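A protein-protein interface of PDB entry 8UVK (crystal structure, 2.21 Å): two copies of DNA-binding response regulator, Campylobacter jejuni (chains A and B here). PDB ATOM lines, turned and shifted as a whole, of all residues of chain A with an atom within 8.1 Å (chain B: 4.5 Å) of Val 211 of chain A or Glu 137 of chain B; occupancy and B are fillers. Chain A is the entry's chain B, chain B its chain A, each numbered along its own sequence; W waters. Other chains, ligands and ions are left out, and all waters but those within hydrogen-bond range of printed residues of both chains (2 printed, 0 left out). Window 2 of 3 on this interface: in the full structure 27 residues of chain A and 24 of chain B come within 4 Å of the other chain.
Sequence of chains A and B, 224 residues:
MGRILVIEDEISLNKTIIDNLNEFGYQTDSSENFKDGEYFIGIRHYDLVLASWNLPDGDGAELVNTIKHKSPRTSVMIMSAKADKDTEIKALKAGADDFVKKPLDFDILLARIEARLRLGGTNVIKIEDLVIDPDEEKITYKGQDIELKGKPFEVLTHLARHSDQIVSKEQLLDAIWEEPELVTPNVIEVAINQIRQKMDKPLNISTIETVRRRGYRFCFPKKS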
ATOM      1  N   GLN A 165     -26.107 -35.596  22.212  1.00  0.00           N
ATOM      2  CA  GLN A 165     -27.073 -34.634  21.706  1.00  0.00           C
ATOM      3  C   GLN A 165     -27.543 -33.776  22.862  1.00  0.00           C
ATOM      4  O   GLN A 165     -27.505 -34.206  24.010  1.00  0.00           O
ATOM      5  CB  GLN A 165     -28.262 -35.341  21.075  1.00  0.00           C
ATOM      6  CG  GLN A 165     -27.902 -36.540  20.218  1.00  0.00           C
ATOM      7  CD  GLN A 165     -29.123 -37.324  19.786  1.00  0.00           C
ATOM      8  OE1 GLN A 165     -30.255 -36.862  19.933  1.00  0.00           O
ATOM      9  NE2 GLN A 165     -28.902 -38.516  19.249  1.00  0.00           N
ATOM     10  N   ILE A 166     -27.994 -32.564  22.568  1.00  0.00           N
ATOM     11  CA  ILE A 166     -28.469 -31.674  23.619  1.00  0.00           C
ATOM     12  C   ILE A 166     -29.961 -31.819  23.837  1.00  0.00           C
ATOM     13  O   ILE A 166     -30.749 -31.585  22.924  1.00  0.00           O
ATOM     14  CB  ILE A 166     -28.171 -30.196  23.304  1.00  0.00           C
ATOM     15  CG1 ILE A 166     -26.668 -29.962  23.182  1.00  0.00           C
ATOM     16  CG2 ILE A 166     -28.755 -29.297  24.381  1.00  0.00           C
ATOM     17  CD1 ILE A 166     -26.309 -28.536  22.827  1.00  0.00           C
ATOM     18  N   VAL A 167     -30.354 -32.204  25.044  1.00  0.00           N
ATOM     19  CA  VAL A 167     -31.770 -32.301  25.358  1.00  0.00           C
ATOM     20  C   VAL A 167     -32.118 -31.154  26.282  1.00  0.00           C
ATOM     21  O   VAL A 167     -31.457 -30.950  27.296  1.00  0.00           O
ATOM     22  CB  VAL A 167     -32.125 -33.645  26.009  1.00  0.00           C
ATOM     23  CG1 VAL A 167     -33.622 -33.733  26.253  1.00  0.00           C
ATOM     24  CG2 VAL A 167     -31.656 -34.796  25.133  1.00  0.00           C
ATOM     25  N   SER A 168     -33.145 -30.393  25.934  1.00  0.00           N
ATOM     26  CA  SER A 168     -33.492 -29.230  26.724  1.00  0.00           C
ATOM     27  C   SER A 168     -34.208 -29.644  28.007  1.00  0.00           C
ATOM     28  O   SER A 168     -34.714 -30.766  28.137  1.00  0.00           O
ATOM     29  CB  SER A 168     -34.354 -28.280  25.888  1.00  0.00           C
ATOM     30  OG  SER A 168     -35.699 -28.748  25.810  1.00  0.00           O
ATOM     31  N   LYS A 169     -34.209 -28.728  28.983  1.00  0.00           N
ATOM     32  CA  LYS A 169     -35.002 -28.966  30.187  1.00  0.00           C
ATOM     33  C   LYS A 169     -36.453 -29.254  29.820  1.00  0.00           C
ATOM     34  O   LYS A 169     -37.092 -30.128  30.422  1.00  0.00           O
ATOM     35  CB  LYS A 169     -34.930 -27.765  31.149  1.00  0.00           C
ATOM     36  CG  LYS A 169     -33.585 -27.620  31.900  1.00  0.00           C
ATOM     37  CD  LYS A 169     -33.668 -26.552  33.012  1.00  0.00           C
ATOM     38  CE  LYS A 169     -33.428 -25.160  32.452  1.00  0.00           C
ATOM     39  NZ  LYS A 169     -31.973 -25.000  32.090  1.00  0.00           N
ATOM     40  N   ARG A 196     -24.919 -36.229  38.992  1.00  0.00           N
ATOM     41  CA  ARG A 196     -23.505 -35.931  39.226  1.00  0.00           C
ATOM     42  C   ARG A 196     -23.091 -36.296  40.654  1.00  0.00           C
ATOM     43  O   ARG A 196     -22.000 -36.840  40.875  1.00  0.00           O
ATOM     44  CB  ARG A 196     -23.233 -34.454  38.919  1.00  0.00           C
ATOM     45  CG  ARG A 196     -23.454 -34.070  37.421  1.00  0.00           C
ATOM     46  CD  ARG A 196     -23.740 -32.562  37.226  1.00  0.00           C
ATOM     47  NE  ARG A 196     -23.476 -32.084  35.864  1.00  0.00           N
ATOM     48  CZ  ARG A 196     -23.832 -30.889  35.400  1.00  0.00           C
ATOM     49  NH1 ARG A 196     -24.523 -30.034  36.143  1.00  0.00           N
ATOM     50  NH2 ARG A 196     -23.507 -30.552  34.154  1.00  0.00           N
ATOM     51  N   ILE A 208     -22.427 -35.734  32.129  1.00  0.00           N
ATOM     52  CA  ILE A 208     -23.419 -34.761  31.708  1.00  0.00           C
ATOM     53  C   ILE A 208     -22.731 -33.415  31.561  1.00  0.00           C
ATOM     54  O   ILE A 208     -22.186 -32.867  32.529  1.00  0.00           O
ATOM     55  CB  ILE A 208     -24.598 -34.669  32.683  1.00  0.00           C
ATOM     56  CG1 ILE A 208     -25.150 -36.060  33.044  1.00  0.00           C
ATOM     57  CG2 ILE A 208     -25.676 -33.810  32.070  1.00  0.00           C
ATOM     58  CD1 ILE A 208     -25.682 -36.850  31.892  1.00  0.00           C
ATOM     59  N   GLU A 209     -22.772 -32.888  30.349  1.00  0.00           N
ATOM     60  CA  GLU A 209     -22.287 -31.563  30.016  1.00  0.00           C
ATOM     61  C   GLU A 209     -23.479 -30.615  29.960  1.00  0.00           C
ATOM     62  O   GLU A 209     -24.479 -30.916  29.305  1.00  0.00           O
ATOM     63  CB  GLU A 209     -21.565 -31.611  28.668  1.00  0.00           C
ATOM     64  CG  GLU A 209     -21.331 -30.274  28.024  1.00  0.00           C
ATOM     65  CD  GLU A 209     -20.445 -30.378  26.787  1.00  0.00           C
ATOM     66  OE1 GLU A 209     -20.602 -31.374  26.021  1.00  0.00           O
ATOM     67  OE2 GLU A 209     -19.563 -29.491  26.618  1.00  0.00           O
ATOM     68  N   THR A 210     -23.381 -29.488  30.648  1.00  0.00           N
ATOM     69  CA  THR A 210     -24.412 -28.463  30.603  1.00  0.00           C
ATOM     70  C   THR A 210     -24.089 -27.499  29.472  1.00  0.00           C
ATOM     71  O   THR A 210     -22.936 -27.085  29.311  1.00  0.00           O
ATOM     72  CB  THR A 210     -24.492 -27.706  31.935  1.00  0.00           C
ATOM     73  OG1 THR A 210     -24.609 -28.635  33.039  1.00  0.00           O
ATOM     74  CG2 THR A 210     -25.690 -26.744  31.950  1.00  0.00           C
ATOM     75  N   VAL A 211     -25.095 -27.142  28.674  1.00  0.00           N
ATOM     76  CA  VAL A 211     -24.873 -26.197  27.588  1.00  0.00           C
ATOM     77  C   VAL A 211     -25.850 -25.051  27.786  1.00  0.00           C
ATOM     78  O   VAL A 211     -27.065 -25.240  27.675  1.00  0.00           O
ATOM     79  CB  VAL A 211     -25.047 -26.823  26.202  1.00  0.00           C
ATOM     80  CG1 VAL A 211     -25.209 -25.695  25.132  1.00  0.00           C
ATOM     81  CG2 VAL A 211     -23.930 -27.837  25.922  1.00  0.00           C
ATOM     82  N   ARG A 212     -25.314 -23.856  28.060  1.00  0.00           N
ATOM     83  CA  ARG A 212     -26.105 -22.742  28.574  1.00  0.00           C
ATOM     84  C   ARG A 212     -27.145 -22.289  27.565  1.00  0.00           C
ATOM     85  O   ARG A 212     -26.812 -22.039  26.402  1.00  0.00           O
ATOM     86  CB  ARG A 212     -25.160 -21.574  28.943  1.00  0.00           C
ATOM     87  CG  ARG A 212     -25.809 -20.390  29.626  1.00  0.00           C
ATOM     88  CD  ARG A 212     -24.797 -19.234  29.698  1.00  0.00           C
ATOM     89  NE  ARG A 212     -25.423 -17.952  29.997  1.00  0.00           N
ATOM     90  CZ  ARG A 212     -25.277 -17.298  31.149  1.00  0.00           C
ATOM     91  NH1 ARG A 212     -24.568 -17.808  32.150  1.00  0.00           N
ATOM     92  NH2 ARG A 212     -25.855 -16.102  31.295  1.00  0.00           N
ATOM     93  N   ARG A 213     -28.389 -22.123  28.045  1.00  0.00           N
ATOM     94  CA  ARG A 213     -29.549 -21.823  27.203  1.00  0.00           C
ATOM     95  C   ARG A 213     -30.033 -22.992  26.316  1.00  0.00           C
ATOM     96  O   ARG A 213     -31.073 -22.862  25.655  1.00  0.00           O
ATOM     97  CB  ARG A 213     -29.275 -20.613  26.307  1.00  0.00           C
ATOM     98  N   ARG A 214     -29.312 -24.114  26.243  1.00  0.00           N
ATOM     99  CA  ARG A 214     -29.765 -25.222  25.397  1.00  0.00           C
ATOM    100  C   ARG A 214     -30.269 -26.397  26.227  1.00  0.00           C
ATOM    101  O   ARG A 214     -31.438 -26.761  26.125  1.00  0.00           O
ATOM    102  CB  ARG A 214     -28.665 -25.695  24.445  1.00  0.00           C
ATOM    103  CG  ARG A 214     -28.070 -24.638  23.570  1.00  0.00           C
ATOM    104  CD  ARG A 214     -28.969 -24.235  22.436  1.00  0.00           C
ATOM    105  NE  ARG A 214     -28.172 -24.073  21.227  1.00  0.00           N
ATOM    106  CZ  ARG A 214     -27.541 -22.960  20.881  1.00  0.00           C
ATOM    107  NH1 ARG A 214     -27.593 -21.869  21.636  1.00  0.00           N
ATOM    108  NH2 ARG A 214     -26.831 -22.941  19.751  1.00  0.00           N
ATOM    109  N   GLY A 215     -29.419 -26.969  27.082  1.00  0.00           N
ATOM    110  CA  GLY A 215     -29.855 -27.919  28.074  1.00  0.00           C
ATOM    111  C   GLY A 215     -28.688 -28.788  28.474  1.00  0.00           C
ATOM    112  O   GLY A 215     -27.609 -28.269  28.793  1.00  0.00           O
ATOM    113  N   TYR A 216     -28.874 -30.111  28.433  1.00  0.00           N
ATOM    114  CA  TYR A 216     -27.861 -31.048  28.890  1.00  0.00           C
ATOM    115  C   TYR A 216     -27.500 -32.023  27.784  1.00  0.00           C
ATOM    116  O   TYR A 216     -28.323 -32.341  26.927  1.00  0.00           O
ATOM    117  CB  TYR A 216     -28.351 -31.803  30.120  1.00  0.00           C
ATOM    118  CG  TYR A 216     -28.655 -30.865  31.249  1.00  0.00           C
ATOM    119  CD1 TYR A 216     -27.670 -30.514  32.165  1.00  0.00           C
ATOM    120  CD2 TYR A 216     -29.926 -30.319  31.393  1.00  0.00           C
ATOM    121  CE1 TYR A 216     -27.948 -29.621  33.220  1.00  0.00           C
ATOM    122  CE2 TYR A 216     -30.217 -29.443  32.423  1.00  0.00           C
ATOM    123  CZ  TYR A 216     -29.223 -29.101  33.345  1.00  0.00           C
ATOM    124  OH  TYR A 216     -29.513 -28.224  34.356  1.00  0.00           O
ATOM    125  N   ARG A 217     -26.260 -32.506  27.807  1.00  0.00           N
ATOM    126  CA  ARG A 217     -25.819 -33.489  26.823  1.00  0.00           C
ATOM    127  C   ARG A 217     -25.019 -34.586  27.497  1.00  0.00           C
ATOM    128  O   ARG A 217     -24.165 -34.310  28.335  1.00  0.00           O
ATOM    129  CB  ARG A 217     -24.958 -32.848  25.737  1.00  0.00           C
ATOM    130  CG  ARG A 217     -24.421 -33.859  24.736  1.00  0.00           C
ATOM    131  CD  ARG A 217     -23.202 -33.358  23.979  1.00  0.00           C
ATOM    132  NE  ARG A 217     -23.514 -32.287  23.040  1.00  0.00           N
ATOM    133  CZ  ARG A 217     -23.271 -31.001  23.267  1.00  0.00           C
ATOM    134  NH1 ARG A 217     -22.706 -30.622  24.404  1.00  0.00           N
ATOM    135  NH2 ARG A 217     -23.584 -30.093  22.354  1.00  0.00           N
ATOM    136  N   ASP B 133     -22.243 -26.553  13.721  1.00  0.00           N
ATOM    137  CA  ASP B 133     -23.526 -27.167  14.049  1.00  0.00           C
ATOM    138  C   ASP B 133     -24.323 -26.325  15.028  1.00  0.00           C
ATOM    139  O   ASP B 133     -24.041 -26.323  16.223  1.00  0.00           O
ATOM    140  CB  ASP B 133     -23.315 -28.567  14.625  1.00  0.00           C
ATOM    141  CG  ASP B 133     -24.619 -29.303  14.869  1.00  0.00           C
ATOM    142  OD1 ASP B 133     -25.692 -28.771  14.518  1.00  0.00           O
ATOM    143  OD2 ASP B 133     -24.566 -30.426  15.409  1.00  0.00           O
ATOM    144  N   PRO B 134     -25.334 -25.616  14.524  1.00  0.00           N
ATOM    145  CA  PRO B 134     -26.164 -24.773  15.384  1.00  0.00           C
ATOM    146  C   PRO B 134     -26.966 -25.593  16.378  1.00  0.00           C
ATOM    147  O   PRO B 134     -27.127 -25.178  17.522  1.00  0.00           O
ATOM    148  CB  PRO B 134     -27.112 -24.092  14.392  1.00  0.00           C
ATOM    149  CG  PRO B 134     -26.451 -24.217  13.060  1.00  0.00           C
ATOM    150  CD  PRO B 134     -25.723 -25.522  13.109  1.00  0.00           C
ATOM    151  N   ASP B 135     -27.460 -26.746  15.950  1.00  0.00           N
ATOM    152  CA  ASP B 135     -28.287 -27.573  16.817  1.00  0.00           C
ATOM    153  C   ASP B 135     -27.548 -27.969  18.083  1.00  0.00           C
ATOM    154  O   ASP B 135     -28.141 -28.033  19.154  1.00  0.00           O
ATOM    155  CB  ASP B 135     -28.744 -28.816  16.058  1.00  0.00           C
ATOM    156  CG  ASP B 135     -29.483 -28.477  14.780  1.00  0.00           C
ATOM    157  OD1 ASP B 135     -29.929 -27.319  14.641  1.00  0.00           O
ATOM    158  OD2 ASP B 135     -29.622 -29.367  13.916  1.00  0.00           O
ATOM    159  N   GLU B 136     -26.255 -28.236  17.964  1.00  0.00           N
ATOM    160  CA  GLU B 136     -25.461 -28.603  19.126  1.00  0.00           C
ATOM    161  C   GLU B 136     -24.548 -27.468  19.550  1.00  0.00           C
ATOM    162  O   GLU B 136     -23.695 -27.649  20.412  1.00  0.00           O
ATOM    163  CB  GLU B 136     -24.638 -29.848  18.820  1.00  0.00           C
ATOM    164  CG  GLU B 136     -25.478 -31.050  18.423  1.00  0.00           C
ATOM    165  CD  GLU B 136     -26.360 -31.544  19.552  1.00  0.00           C
ATOM    166  OE1 GLU B 136     -25.873 -31.623  20.698  1.00  0.00           O
ATOM    167  OE2 GLU B 136     -27.543 -31.845  19.293  1.00  0.00           O
ATOM    168  N   GLU B 137     -24.722 -26.297  18.946  1.00  0.00           N
ATOM    169  CA  GLU B 137     -23.858 -25.158  19.247  1.00  0.00           C
ATOM    170  C   GLU B 137     -22.408 -25.596  19.242  1.00  0.00           C
ATOM    171  O   GLU B 137     -21.680 -25.374  20.206  1.00  0.00           O
ATOM    172  CB  GLU B 137     -24.212 -24.521  20.590  1.00  0.00           C
ATOM    173  CG  GLU B 137     -23.671 -23.108  20.752  1.00  0.00           C
ATOM    174  CD  GLU B 137     -23.987 -22.509  22.107  1.00  0.00           C
ATOM    175  OE1 GLU B 137     -24.245 -23.279  23.055  1.00  0.00           O
ATOM    176  OE2 GLU B 137     -23.983 -21.267  22.225  1.00  0.00           O
ATOM    177  N   LYS B 138     -21.988 -26.227  18.155  1.00  0.00           N
ATOM    178  CA  LYS B 138     -20.619 -26.711  18.080  1.00  0.00           C
ATOM    179  C   LYS B 138     -19.891 -26.306  16.817  1.00  0.00           C
ATOM    180  O   LYS B 138     -20.462 -26.322  15.730  1.00  0.00           O
ATOM    181  CB  LYS B 138     -20.583 -28.236  18.212  1.00  0.00           C
ATOM    182  CG  LYS B 138     -20.764 -28.743  19.631  1.00  0.00           C
ATOM    183  CD  LYS B 138     -20.640 -30.256  19.687  1.00  0.00           C
ATOM    184  CE  LYS B 138     -20.671 -30.762  21.119  1.00  0.00           C
ATOM    185  NZ  LYS B 138     -20.627 -32.248  21.184  1.00  0.00           N
ATOM    186  N   ILE B 139     -18.630 -25.929  16.961  1.00  0.00           N
ATOM    187  CA  ILE B 139     -17.800 -25.585  15.818  1.00  0.00           C
ATOM    188  C   ILE B 139     -16.552 -26.440  15.912  1.00  0.00           C
ATOM    189  O   ILE B 139     -15.925 -26.500  16.972  1.00  0.00           O
ATOM    190  CB  ILE B 139     -17.392 -24.099  15.793  1.00  0.00           C
ATOM    191  CG1 ILE B 139     -18.602 -23.194  15.868  1.00  0.00           C
ATOM    192  CG2 ILE B 139     -16.687 -23.794  14.500  1.00  0.00           C
ATOM    193  CD1 ILE B 139     -18.235 -21.765  16.110  1.00  0.00           C
ATOM    194  N   LYS B 149     -19.404 -19.593  21.525  1.00  0.00           N
ATOM    195  CA  LYS B 149     -20.793 -19.799  21.900  1.00  0.00           C
ATOM    196  C   LYS B 149     -21.559 -18.503  22.041  1.00  0.00           C
ATOM    197  O   LYS B 149     -21.028 -17.427  21.781  1.00  0.00           O
ATOM    198  CB  LYS B 149     -20.867 -20.574  23.215  1.00  0.00           C
ATOM    199  N   GLY B 150     -22.818 -18.604  22.441  1.00  0.00           N
ATOM    200  CA  GLY B 150     -23.623 -17.419  22.643  1.00  0.00           C
ATOM    201  C   GLY B 150     -23.793 -16.581  21.404  1.00  0.00           C
ATOM    202  O   GLY B 150     -23.717 -17.083  20.285  1.00  0.00           O
ATOM    203  N   PHE B 153     -21.463 -16.949  18.550  1.00  0.00           N
ATOM    204  CA  PHE B 153     -21.824 -18.128  17.768  1.00  0.00           C
ATOM    205  C   PHE B 153     -22.921 -17.810  16.765  1.00  0.00           C
ATOM    206  O   PHE B 153     -22.834 -18.207  15.601  1.00  0.00           O
ATOM    207  CB  PHE B 153     -22.263 -19.278  18.686  1.00  0.00           C
ATOM    208  CG  PHE B 153     -22.479 -20.588  17.958  1.00  0.00           C
ATOM    209  CD1 PHE B 153     -23.709 -20.880  17.359  1.00  0.00           C
ATOM    210  CD2 PHE B 153     -21.451 -21.521  17.854  1.00  0.00           C
ATOM    211  CE1 PHE B 153     -23.913 -22.094  16.660  1.00  0.00           C
ATOM    212  CE2 PHE B 153     -21.645 -22.737  17.154  1.00  0.00           C
ATOM    213  CZ  PHE B 153     -22.875 -23.018  16.552  1.00  0.00           C
HETATM  214  O   HOH W   1     -21.921 -27.237  22.464  1.00  0.00           O
HETATM  215  O   HOH W   2     -24.108 -22.445  26.063  1.00  0.00           O
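The guanidinium group of Arg 214 of chain A is in hydrogen-bond range of the backbone carbonyl oxygen of Pro 134 of chain B, at 3.2 Å.
The side-chain carboxylate (OE2) of Glu 137 of chain B is in salt-bridge range of the guanidinium group (NH1) of Arg 214 of chain A (3.7 Å).
The side-chain amino group (NZ) of Lys 138 of chain B sits close to the guanidinium group (NE) of Arg 217 of chain A (3.4 Å).
The side-chain carboxylate of Glu 136 of chain B lies within hydrogen-bond range of the backbone NH of Ile 166 of chain A, 3.0 Å away.
OE1 of Glu 136 of chain B lies within salt-bridge range of NH2 of Arg 217 of chain A, at 3.2 Å.
No position is printed for both chains.
Of the 7 pairs that touch across the chains among the printed residues, none has its exchanged pair printed and touching as well.
Of the 16 printed residues of chain A, 5 touch a printed residue of chain B.
Hydrophobic or aromatic side chains of chain A within 4 Å of the printed part of chain B: Ile 166 and Val 211.
Among the printed residues, 7 pairs touch across the chains.
Among the printed residues, Asp or Glu carboxylates within 4 Å of a Lys or Arg side-chain nitrogen of the other chain: Arg 214 of chain A with Glu 137 of chain B (3.7 Å) and Arg 217 of chain A with Glu 136 of chain B (3.2 Å).
The side-chain carboxylate (OE2) of Glu 137 of chain B sits at hydrogen-bond distance from the backbone NH (N) of Gly 150 of chain B (2.9 Å).
The guanidinium group of Arg 217 of chain A lies within salt-bridge range of the side-chain carboxylate of Glu 209 of chain A, 2.8 Å away.
The backbone NH (N) of Asp 133 of chain B sits at hydrogen-bond distance from the backbone carbonyl oxygen (O) of Lys 138 of chain B, 2.7 Å away.
Printed residues of chain B within 4 Å of Gln 165 of chain A: Glu 136 (3.4 Å).
Of the printed residues of chain B, Ile 166 of chain A touches Glu 136 (3.0 Å).
Of chain B, only Glu 137 comes within 4 Å of Val 211 of chain A.
Asp 133 of chain B touches none of the printed residues of chain A.
Glu 137 of chain B touches just these residues of chain A: Val 211 and Arg 214.
Printed residues of chain A within 4 Å of Lys 138 of chain B: Arg 217.
Lys 149 of chain B touches none of the printed residues of chain A.
The nearest printed residue of chain B that does not touch Val 211 of chain A is Glu 136 of chain B (5.3 Å).
The nearest residue of chain A that does not touch Glu 137 of chain B is Arg 212 of chain A (4.4 Å).
The nearest printed residue of chain B that does not touch Arg 214 of chain A is Phe 153 of chain B (4.3 Å).
Water W2 bridges N of Arg 212 of chain A (2.7 Å) and OE1 of Glu 137 of chain B (3.1 Å).
Water W1 lies within hydrogen-bond range of O of Glu 136 of chain B (2.7 Å), O of Glu 137 of chain B (2.9 Å) and NH2 of Arg 217 of chain A (3.3 Å).
Glu 136 of chain B touches Gln 165 of chain A.
Val 211 of chain A touches Glu 137 of chain B (CG1 to OE1, 3.3 Å).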
